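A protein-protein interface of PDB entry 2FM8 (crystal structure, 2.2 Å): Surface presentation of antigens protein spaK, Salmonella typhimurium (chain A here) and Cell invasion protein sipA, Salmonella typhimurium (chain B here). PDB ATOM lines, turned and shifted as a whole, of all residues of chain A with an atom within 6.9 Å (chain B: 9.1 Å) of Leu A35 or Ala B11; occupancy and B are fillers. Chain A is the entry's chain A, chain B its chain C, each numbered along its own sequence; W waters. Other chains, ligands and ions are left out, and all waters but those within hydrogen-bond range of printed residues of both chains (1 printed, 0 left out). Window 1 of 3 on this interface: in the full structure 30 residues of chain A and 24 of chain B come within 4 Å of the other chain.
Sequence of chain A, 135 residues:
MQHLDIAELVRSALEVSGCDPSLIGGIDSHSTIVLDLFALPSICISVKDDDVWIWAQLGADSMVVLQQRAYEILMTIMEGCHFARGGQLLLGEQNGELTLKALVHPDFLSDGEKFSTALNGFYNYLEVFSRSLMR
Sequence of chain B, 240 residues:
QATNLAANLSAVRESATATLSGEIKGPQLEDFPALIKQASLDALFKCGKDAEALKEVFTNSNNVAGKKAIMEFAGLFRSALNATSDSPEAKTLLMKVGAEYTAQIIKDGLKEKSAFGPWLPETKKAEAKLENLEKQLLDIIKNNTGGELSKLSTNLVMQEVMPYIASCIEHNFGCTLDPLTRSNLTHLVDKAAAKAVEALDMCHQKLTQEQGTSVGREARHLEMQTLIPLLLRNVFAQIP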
ATOM      1  N   VAL A  10      -3.443  25.637 -25.020  1.00  0.00           N
ATOM      2  CA  VAL A  10      -4.032  25.138 -23.784  1.00  0.00           C
ATOM      3  C   VAL A  10      -3.011  24.255 -23.032  1.00  0.00           C
ATOM      4  O   VAL A  10      -2.811  24.399 -21.831  1.00  0.00           O
ATOM      5  CB  VAL A  10      -5.331  24.355 -24.087  1.00  0.00           C
ATOM      6  CG1 VAL A  10      -5.788  23.541 -22.889  1.00  0.00           C
ATOM      7  CG2 VAL A  10      -6.443  25.325 -24.512  1.00  0.00           C
ATOM      8  N   LEU A  14      -1.457  25.177 -19.288  1.00  0.00           N
ATOM      9  CA  LEU A  14      -1.680  24.276 -18.170  1.00  0.00           C
ATOM     10  C   LEU A  14      -0.360  23.829 -17.592  1.00  0.00           C
ATOM     11  O   LEU A  14      -0.257  23.642 -16.382  1.00  0.00           O
ATOM     12  CB  LEU A  14      -2.528  23.076 -18.586  1.00  0.00           C
ATOM     13  CG  LEU A  14      -3.973  23.406 -18.980  1.00  0.00           C
ATOM     14  CD1 LEU A  14      -4.622  22.131 -19.509  1.00  0.00           C
ATOM     15  CD2 LEU A  14      -4.788  23.999 -17.830  1.00  0.00           C
ATOM     16  N   LEU A  23      -3.437  14.259 -16.820  1.00  0.00           N
ATOM     17  CA  LEU A  23      -4.900  14.535 -16.831  1.00  0.00           C
ATOM     18  C   LEU A  23      -5.459  14.957 -18.192  1.00  0.00           C
ATOM     19  O   LEU A  23      -6.683  14.930 -18.414  1.00  0.00           O
ATOM     20  CB  LEU A  23      -5.249  15.628 -15.821  1.00  0.00           C
ATOM     21  CG  LEU A  23      -4.915  15.305 -14.367  1.00  0.00           C
ATOM     22  CD1 LEU A  23      -5.375  16.404 -13.454  1.00  0.00           C
ATOM     23  CD2 LEU A  23      -5.538  13.966 -13.947  1.00  0.00           C
ATOM     24  N   ILE A  24      -4.550  15.351 -19.075  1.00  0.00           N
ATOM     25  CA  ILE A  24      -4.868  15.846 -20.385  1.00  0.00           C
ATOM     26  C   ILE A  24      -5.109  14.693 -21.384  1.00  0.00           C
ATOM     27  O   ILE A  24      -4.180  13.955 -21.741  1.00  0.00           O
ATOM     28  CB  ILE A  24      -3.719  16.768 -20.896  1.00  0.00           C
ATOM     29  CG1 ILE A  24      -3.482  17.930 -19.927  1.00  0.00           C
ATOM     30  CG2 ILE A  24      -4.037  17.317 -22.302  1.00  0.00           C
ATOM     31  CD1 ILE A  24      -2.236  18.759 -20.242  1.00  0.00           C
ATOM     32  N   GLY A  25      -6.355  14.552 -21.832  1.00  0.00           N
ATOM     33  CA  GLY A  25      -6.715  13.516 -22.788  1.00  0.00           C
ATOM     34  C   GLY A  25      -6.451  13.918 -24.233  1.00  0.00           C
ATOM     35  O   GLY A  25      -5.574  14.748 -24.525  1.00  0.00           O
ATOM     36  N   ILE A  33     -12.529  22.203 -26.188  1.00  0.00           N
ATOM     37  CA  ILE A  33     -11.724  21.639 -25.113  1.00  0.00           C
ATOM     38  C   ILE A  33     -12.441  21.929 -23.795  1.00  0.00           C
ATOM     39  O   ILE A  33     -12.943  23.038 -23.583  1.00  0.00           O
ATOM     40  CB  ILE A  33     -10.327  22.263 -25.095  1.00  0.00           C
ATOM     41  CG1 ILE A  33      -9.593  21.909 -26.377  1.00  0.00           C
ATOM     42  CG2 ILE A  33      -9.514  21.784 -23.899  1.00  0.00           C
ATOM     43  CD1 ILE A  33      -8.326  22.649 -26.563  1.00  0.00           C
ATOM     44  N   VAL A  34     -12.514  20.921 -22.935  1.00  0.00           N
ATOM     45  CA  VAL A  34     -13.234  21.014 -21.679  1.00  0.00           C
ATOM     46  C   VAL A  34     -12.273  20.696 -20.528  1.00  0.00           C
ATOM     47  O   VAL A  34     -11.609  19.655 -20.550  1.00  0.00           O
ATOM     48  CB  VAL A  34     -14.451  20.069 -21.638  1.00  0.00           C
ATOM     49  CG1 VAL A  34     -15.198  20.224 -20.311  1.00  0.00           C
ATOM     50  CG2 VAL A  34     -15.392  20.373 -22.784  1.00  0.00           C
ATOM     51  N   LEU A  35     -12.196  21.606 -19.562  1.00  0.00           N
ATOM     52  CA  LEU A  35     -11.501  21.385 -18.278  1.00  0.00           C
ATOM     53  C   LEU A  35     -12.510  21.084 -17.176  1.00  0.00           C
ATOM     54  O   LEU A  35     -13.270  21.981 -16.769  1.00  0.00           O
ATOM     55  CB  LEU A  35     -10.715  22.639 -17.864  1.00  0.00           C
ATOM     56  CG  LEU A  35      -9.893  23.395 -18.912  1.00  0.00           C
ATOM     57  CD1 LEU A  35      -9.116  24.478 -18.231  1.00  0.00           C
ATOM     58  CD2 LEU A  35      -8.977  22.483 -19.645  1.00  0.00           C
ATOM     59  N   ASP A  36     -12.572  19.830 -16.742  1.00  0.00           N
ATOM     60  CA  ASP A  36     -13.412  19.453 -15.608  1.00  0.00           C
ATOM     61  C   ASP A  36     -12.664  19.817 -14.325  1.00  0.00           C
ATOM     62  O   ASP A  36     -11.448  19.692 -14.265  1.00  0.00           O
ATOM     63  CB  ASP A  36     -13.743  17.957 -15.596  1.00  0.00           C
ATOM     64  CG  ASP A  36     -14.575  17.517 -16.799  1.00  0.00           C
ATOM     65  OD1 ASP A  36     -15.640  18.135 -17.063  1.00  0.00           O
ATOM     66  OD2 ASP A  36     -14.145  16.554 -17.482  1.00  0.00           O
ATOM     67  N   LEU A  37     -13.426  20.228 -13.318  1.00  0.00           N
ATOM     68  CA  LEU A  37     -12.914  20.779 -12.082  1.00  0.00           C
ATOM     69  C   LEU A  37     -13.578  20.180 -10.856  1.00  0.00           C
ATOM     70  O   LEU A  37     -14.732  19.758 -10.894  1.00  0.00           O
ATOM     71  CB  LEU A  37     -13.169  22.292 -12.063  1.00  0.00           C
ATOM     72  CG  LEU A  37     -12.541  23.122 -13.178  1.00  0.00           C
ATOM     73  CD1 LEU A  37     -12.986  24.563 -13.031  1.00  0.00           C
ATOM     74  CD2 LEU A  37     -11.017  23.026 -13.144  1.00  0.00           C
ATOM     75  N   LEU A  40     -16.457  22.942  -9.256  1.00  0.00           N
ATOM     76  CA  LEU A  40     -16.906  24.046 -10.065  1.00  0.00           C
ATOM     77  C   LEU A  40     -17.392  23.563 -11.428  1.00  0.00           C
ATOM     78  O   LEU A  40     -17.006  22.485 -11.905  1.00  0.00           O
ATOM     79  CB  LEU A  40     -15.767  25.034 -10.289  1.00  0.00           C
ATOM     80  CG  LEU A  40     -15.288  25.789  -9.057  1.00  0.00           C
ATOM     81  CD1 LEU A  40     -14.025  26.577  -9.388  1.00  0.00           C
ATOM     82  CD2 LEU A  40     -16.382  26.720  -8.542  1.00  0.00           C
ATOM     83  N   PRO A  41     -18.212  24.383 -12.080  1.00  0.00           N
ATOM     84  CA  PRO A  41     -18.582  24.055 -13.442  1.00  0.00           C
ATOM     85  C   PRO A  41     -17.335  23.901 -14.325  1.00  0.00           C
ATOM     86  O   PRO A  41     -16.331  24.577 -14.101  1.00  0.00           O
ATOM     87  CB  PRO A  41     -19.405  25.269 -13.881  1.00  0.00           C
ATOM     88  CG  PRO A  41     -19.890  25.883 -12.600  1.00  0.00           C
ATOM     89  CD  PRO A  41     -18.795  25.662 -11.641  1.00  0.00           C
ATOM     90  N   SER A  42     -17.416  23.013 -15.301  1.00  0.00           N
ATOM     91  CA  SER A  42     -16.372  22.864 -16.286  1.00  0.00           C
ATOM     92  C   SER A  42     -16.131  24.133 -17.146  1.00  0.00           C
ATOM     93  O   SER A  42     -17.046  24.874 -17.483  1.00  0.00           O
ATOM     94  CB  SER A  42     -16.648  21.639 -17.159  1.00  0.00           C
ATOM     95  OG  SER A  42     -16.790  20.484 -16.335  1.00  0.00           O
ATOM     96  N   ILE A  43     -14.854  24.367 -17.457  1.00  0.00           N
ATOM     97  CA  ILE A  43     -14.436  25.440 -18.344  1.00  0.00           C
ATOM     98  C   ILE A  43     -14.274  24.903 -19.782  1.00  0.00           C
ATOM     99  O   ILE A  43     -13.579  23.892 -20.016  1.00  0.00           O
ATOM    100  CB  ILE A  43     -13.144  26.056 -17.836  1.00  0.00           C
ATOM    101  CG1 ILE A  43     -13.374  26.625 -16.432  1.00  0.00           C
ATOM    102  CG2 ILE A  43     -12.587  27.096 -18.846  1.00  0.00           C
ATOM    103  CD1 ILE A  43     -12.120  27.188 -15.744  1.00  0.00           C
ATOM    104  N   CYS A  44     -14.942  25.567 -20.725  1.00  0.00           N
ATOM    105  CA  CYS A  44     -14.861  25.247 -22.138  1.00  0.00           C
ATOM    106  C   CYS A  44     -14.023  26.288 -22.848  1.00  0.00           C
ATOM    107  O   CYS A  44     -14.103  27.483 -22.562  1.00  0.00           O
ATOM    108  CB  CYS A  44     -16.237  25.175 -22.784  1.00  0.00           C
ATOM    109  SG  CYS A  44     -17.371  24.002 -22.005  1.00  0.00           S
ATOM    110  N   ILE A  45     -13.204  25.804 -23.775  1.00  0.00           N
ATOM    111  CA  ILE A  45     -12.390  26.650 -24.616  1.00  0.00           C
ATOM    112  C   ILE A  45     -12.687  26.327 -26.068  1.00  0.00           C
ATOM    113  O   ILE A  45     -12.626  25.164 -26.479  1.00  0.00           O
ATOM    114  CB  ILE A  45     -10.903  26.467 -24.359  1.00  0.00           C
ATOM    115  CG1 ILE A  45     -10.613  26.630 -22.859  1.00  0.00           C
ATOM    116  CG2 ILE A  45     -10.116  27.485 -25.219  1.00  0.00           C
ATOM    117  CD1 ILE A  45      -9.521  25.832 -22.359  1.00  0.00           C
ATOM    118  N   LEU A 119      -6.633  31.940 -18.470  1.00  0.00           N
ATOM    119  CA  LEU A 119      -7.340  30.780 -17.924  1.00  0.00           C
ATOM    120  C   LEU A 119      -7.482  30.809 -16.403  1.00  0.00           C
ATOM    121  O   LEU A 119      -8.522  30.430 -15.864  1.00  0.00           O
ATOM    122  CB  LEU A 119      -6.657  29.452 -18.304  1.00  0.00           C
ATOM    123  CG  LEU A 119      -6.815  28.902 -19.716  1.00  0.00           C
ATOM    124  CD1 LEU A 119      -5.962  27.593 -19.877  1.00  0.00           C
ATOM    125  CD2 LEU A 119      -8.239  28.637 -20.041  1.00  0.00           C
ATOM    126  N   LEU B   5      -6.448  26.569 -10.296  1.00  0.00           N
ATOM    127  CA  LEU B   5      -6.988  25.799 -11.418  1.00  0.00           C
ATOM    128  C   LEU B   5      -6.247  24.473 -11.577  1.00  0.00           C
ATOM    129  O   LEU B   5      -6.869  23.414 -11.698  1.00  0.00           O
ATOM    130  CB  LEU B   5      -6.897  26.628 -12.706  1.00  0.00           C
ATOM    131  CG  LEU B   5      -7.048  25.961 -14.071  1.00  0.00           C
ATOM    132  CD1 LEU B   5      -8.394  25.310 -14.218  1.00  0.00           C
ATOM    133  CD2 LEU B   5      -6.897  27.049 -15.132  1.00  0.00           C
ATOM    134  N   ALA B   6      -4.925  24.522 -11.575  1.00  0.00           N
ATOM    135  CA  ALA B   6      -4.124  23.315 -11.727  1.00  0.00           C
ATOM    136  C   ALA B   6      -4.382  22.307 -10.588  1.00  0.00           C
ATOM    137  O   ALA B   6      -4.553  21.092 -10.828  1.00  0.00           O
ATOM    138  CB  ALA B   6      -2.641  23.682 -11.803  1.00  0.00           C
ATOM    139  N   ASN B   8      -7.011  22.016  -8.888  1.00  0.00           N
ATOM    140  CA  ASN B   8      -8.388  21.545  -8.870  1.00  0.00           C
ATOM    141  C   ASN B   8      -8.831  20.902 -10.190  1.00  0.00           C
ATOM    142  O   ASN B   8     -10.008  20.578 -10.358  1.00  0.00           O
ATOM    143  CB  ASN B   8      -9.301  22.703  -8.465  1.00  0.00           C
ATOM    144  CG  ASN B   8      -9.137  23.058  -7.008  1.00  0.00           C
ATOM    145  OD1 ASN B   8      -8.475  24.053  -6.631  1.00  0.00           O
ATOM    146  ND2 ASN B   8      -9.666  22.211  -6.175  1.00  0.00           N
ATOM    147  N   LEU B   9      -7.873  20.687 -11.088  1.00  0.00           N
ATOM    148  CA  LEU B   9      -8.151  20.161 -12.400  1.00  0.00           C
ATOM    149  C   LEU B   9      -8.410  18.683 -12.279  1.00  0.00           C
ATOM    150  O   LEU B   9      -7.663  17.946 -11.652  1.00  0.00           O
ATOM    151  CB  LEU B   9      -6.995  20.401 -13.364  1.00  0.00           C
ATOM    152  CG  LEU B   9      -7.299  19.996 -14.808  1.00  0.00           C
ATOM    153  CD1 LEU B   9      -8.172  21.047 -15.458  1.00  0.00           C
ATOM    154  CD2 LEU B   9      -5.999  19.808 -15.570  1.00  0.00           C
ATOM    155  N   SER B  10      -9.497  18.258 -12.872  1.00  0.00           N
ATOM    156  CA  SER B  10      -9.956  16.922 -12.672  1.00  0.00           C
ATOM    157  C   SER B  10      -9.797  16.096 -13.973  1.00  0.00           C
ATOM    158  O   SER B  10      -9.569  14.873 -13.931  1.00  0.00           O
ATOM    159  CB  SER B  10     -11.390  17.016 -12.120  1.00  0.00           C
ATOM    160  OG  SER B  10     -12.021  15.791 -12.331  1.00  0.00           O
ATOM    161  N   ALA B  11      -9.881  16.775 -15.120  1.00  0.00           N
ATOM    162  CA  ALA B  11      -9.580  16.194 -16.456  1.00  0.00           C
ATOM    163  C   ALA B  11      -9.548  17.278 -17.536  1.00  0.00           C
ATOM    164  O   ALA B  11     -10.143  18.328 -17.376  1.00  0.00           O
ATOM    165  CB  ALA B  11     -10.595  15.121 -16.838  1.00  0.00           C
ATOM    166  N   VAL B  12      -8.854  17.004 -18.631  1.00  0.00           N
ATOM    167  CA  VAL B  12      -8.964  17.775 -19.865  1.00  0.00           C
ATOM    168  C   VAL B  12      -9.408  16.841 -20.997  1.00  0.00           C
ATOM    169  O   VAL B  12      -8.792  15.775 -21.260  1.00  0.00           O
ATOM    170  CB  VAL B  12      -7.654  18.448 -20.238  1.00  0.00           C
ATOM    171  CG1 VAL B  12      -7.851  19.375 -21.452  1.00  0.00           C
ATOM    172  CG2 VAL B  12      -7.103  19.231 -19.042  1.00  0.00           C
ATOM    173  N   ARG B  13     -10.519  17.208 -21.627  1.00  0.00           N
ATOM    174  CA  ARG B  13     -11.084  16.394 -22.680  1.00  0.00           C
ATOM    175  C   ARG B  13     -11.634  17.282 -23.762  1.00  0.00           C
ATOM    176  O   ARG B  13     -11.597  18.504 -23.657  1.00  0.00           O
ATOM    177  CB  ARG B  13     -12.186  15.485 -22.123  1.00  0.00           C
ATOM    178  CG  ARG B  13     -13.326  16.211 -21.417  1.00  0.00           C
ATOM    179  CD  ARG B  13     -14.286  15.241 -20.739  1.00  0.00           C
ATOM    180  NE  ARG B  13     -15.223  15.958 -19.881  1.00  0.00           N
ATOM    181  CZ  ARG B  13     -16.373  16.497 -20.286  1.00  0.00           C
ATOM    182  NH1 ARG B  13     -16.793  16.344 -21.538  1.00  0.00           N
ATOM    183  NH2 ARG B  13     -17.114  17.204 -19.421  1.00  0.00           N
ATOM    184  N   GLU B  14     -12.130  16.669 -24.822  1.00  0.00           N
ATOM    185  CA  GLU B  14     -12.823  17.420 -25.831  1.00  0.00           C
ATOM    186  C   GLU B  14     -14.259  16.952 -25.943  1.00  0.00           C
ATOM    187  O   GLU B  14     -14.616  15.857 -25.497  1.00  0.00           O
ATOM    188  CB  GLU B  14     -12.090  17.374 -27.174  1.00  0.00           C
ATOM    189  CG  GLU B  14     -11.896  16.026 -27.772  1.00  0.00           C
ATOM    190  CD  GLU B  14     -10.923  16.054 -28.961  1.00  0.00           C
ATOM    191  OE1 GLU B  14     -10.475  17.173 -29.356  1.00  0.00           O
ATOM    192  OE2 GLU B  14     -10.602  14.956 -29.485  1.00  0.00           O
ATOM    193  N   SER B  15     -15.074  17.816 -26.526  1.00  0.00           N
ATOM    194  CA  SER B  15     -16.482  17.580 -26.652  1.00  0.00           C
ATOM    195  C   SER B  15     -16.952  18.095 -27.997  1.00  0.00           C
ATOM    196  O   SER B  15     -16.680  19.243 -28.370  1.00  0.00           O
ATOM    197  CB  SER B  15     -17.228  18.288 -25.517  1.00  0.00           C
ATOM    198  OG  SER B  15     -18.580  18.500 -25.854  1.00  0.00           O
ATOM    199  N   ALA B  18     -20.419  20.248 -26.588  1.00  0.00           N
ATOM    200  CA  ALA B  18     -20.260  21.550 -25.940  1.00  0.00           C
ATOM    201  C   ALA B  18     -20.039  22.641 -26.966  1.00  0.00           C
ATOM    202  O   ALA B  18     -19.064  22.622 -27.698  1.00  0.00           O
ATOM    203  CB  ALA B  18     -19.101  21.518 -24.972  1.00  0.00           C
HETATM  204  O   HOH W   1     -14.346  16.599 -10.471  1.00  0.00           O
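The backbone NH of Val B12 is in hydrogen-bond range of the backbone carbonyl oxygen of Leu A23 (3.0 Å).
The backbone NH (N) of Gly A25 lies within hydrogen-bond range of the backbone carbonyl oxygen (O) of Val B12.
The backbone carbonyl oxygen of Arg B13 lies within hydrogen-bond range of the backbone NH of Val A34, at 2.7 Å.
N of Ser B10 is in hydrogen-bond range of O of Asp A36, 2.8 Å away.
N of Asp A36 is in hydrogen-bond range of O of Ala B11, at 2.9 Å.
NE of Arg B13 is in salt-bridge range of OD2 of Asp A36 (2.7 Å).
O of Ile A33 sits at hydrogen-bond distance from N of Ile A45 (2.8 Å).
The backbone carbonyl oxygen of Ile A43 sits at hydrogen-bond distance from the backbone NH of Leu A35, at 2.7 Å.
The side-chain carboxylate (OD1) of Asp A36 is in hydrogen-bond range of the side-chain hydroxyl (OG) of Ser A42.
OG of Ser B15 is in hydrogen-bond range of N of Ala B18.
Val B12 touches Leu A14 (CG2 to CD1, 3.8 Å).
Leu A23 touches Ala B11.
Ile A24 touches Val B12 (CA to CB, 3.8 Å).
Val A34 touches Ala B11 (O to O, 3.7 Å).
Val B12 touches Val A34 (CA to O, 3.3 Å).
Val A34 touches Ser B15.
CB of Leu A35 touches CD1 of Leu B9, at 3.8 Å.
Leu A35 touches Ala B11 (CA to O, 3.5 Å).
Leu A35 touches Val B12 (CD2 to CG1, 3.8 Å).
CD2 of Leu B5 touches O of Leu A119 (3.8 Å).
Of the printed residues of chain B, Gly A25 touches Val B12 (2.8 Å).
Of chain B, only Ala B11, Val B12, Arg B13 and Ser B15 come within 4 Å of Val A34.
Leu A35 touches just these residues of chain B: Leu B9, Ala B11 and Val B12.
Pro A41 touches none of the printed residues of chain B.
Ser A42 touches none of the printed residues of chain B.
Cys A44 touches none of the printed residues of chain B.
Printed residues of chain B within 4 Å of Leu A119: Leu B5 (3.8 Å).
Printed residues of chain A within 4 Å of Ser B10: Asp A36 (2.8 Å) and Leu A37 (3.99 Å).
Printed residues of chain A within 4 Å of Arg B13: Ile A33, Val A34 and Asp A36.
The nearest residue of chain A that does not touch Ala B11 is Leu A37 (5.3 Å).
Printed residues of chain B that touch a printed residue of chain A: Leu B5, Asn B8, Leu B9, Ser B10, Ala B11, Val B12, Arg B13 and Ser B15.
Of the 17 printed residues of chain A, 10 touch a printed residue of chain B.
Hydrophobic or aromatic side chains of chain A that line the printed part of chain B: Leu A14, Leu A23, Ile A24, Ile A33, Val A34, Leu A35, Leu A37 and Leu A119.
Among the printed residues, 23 pairs touch across the chains.
Among the printed residues, Asp or Glu carboxylates within 4 Å of a Lys or Arg side-chain nitrogen of the other chain: Asp A36 with Arg B13 (2.7 Å).
Water W1 lies within hydrogen-bond range of OG of Ser B10 (3.1 Å) and O of Leu A37 (3.2 Å).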
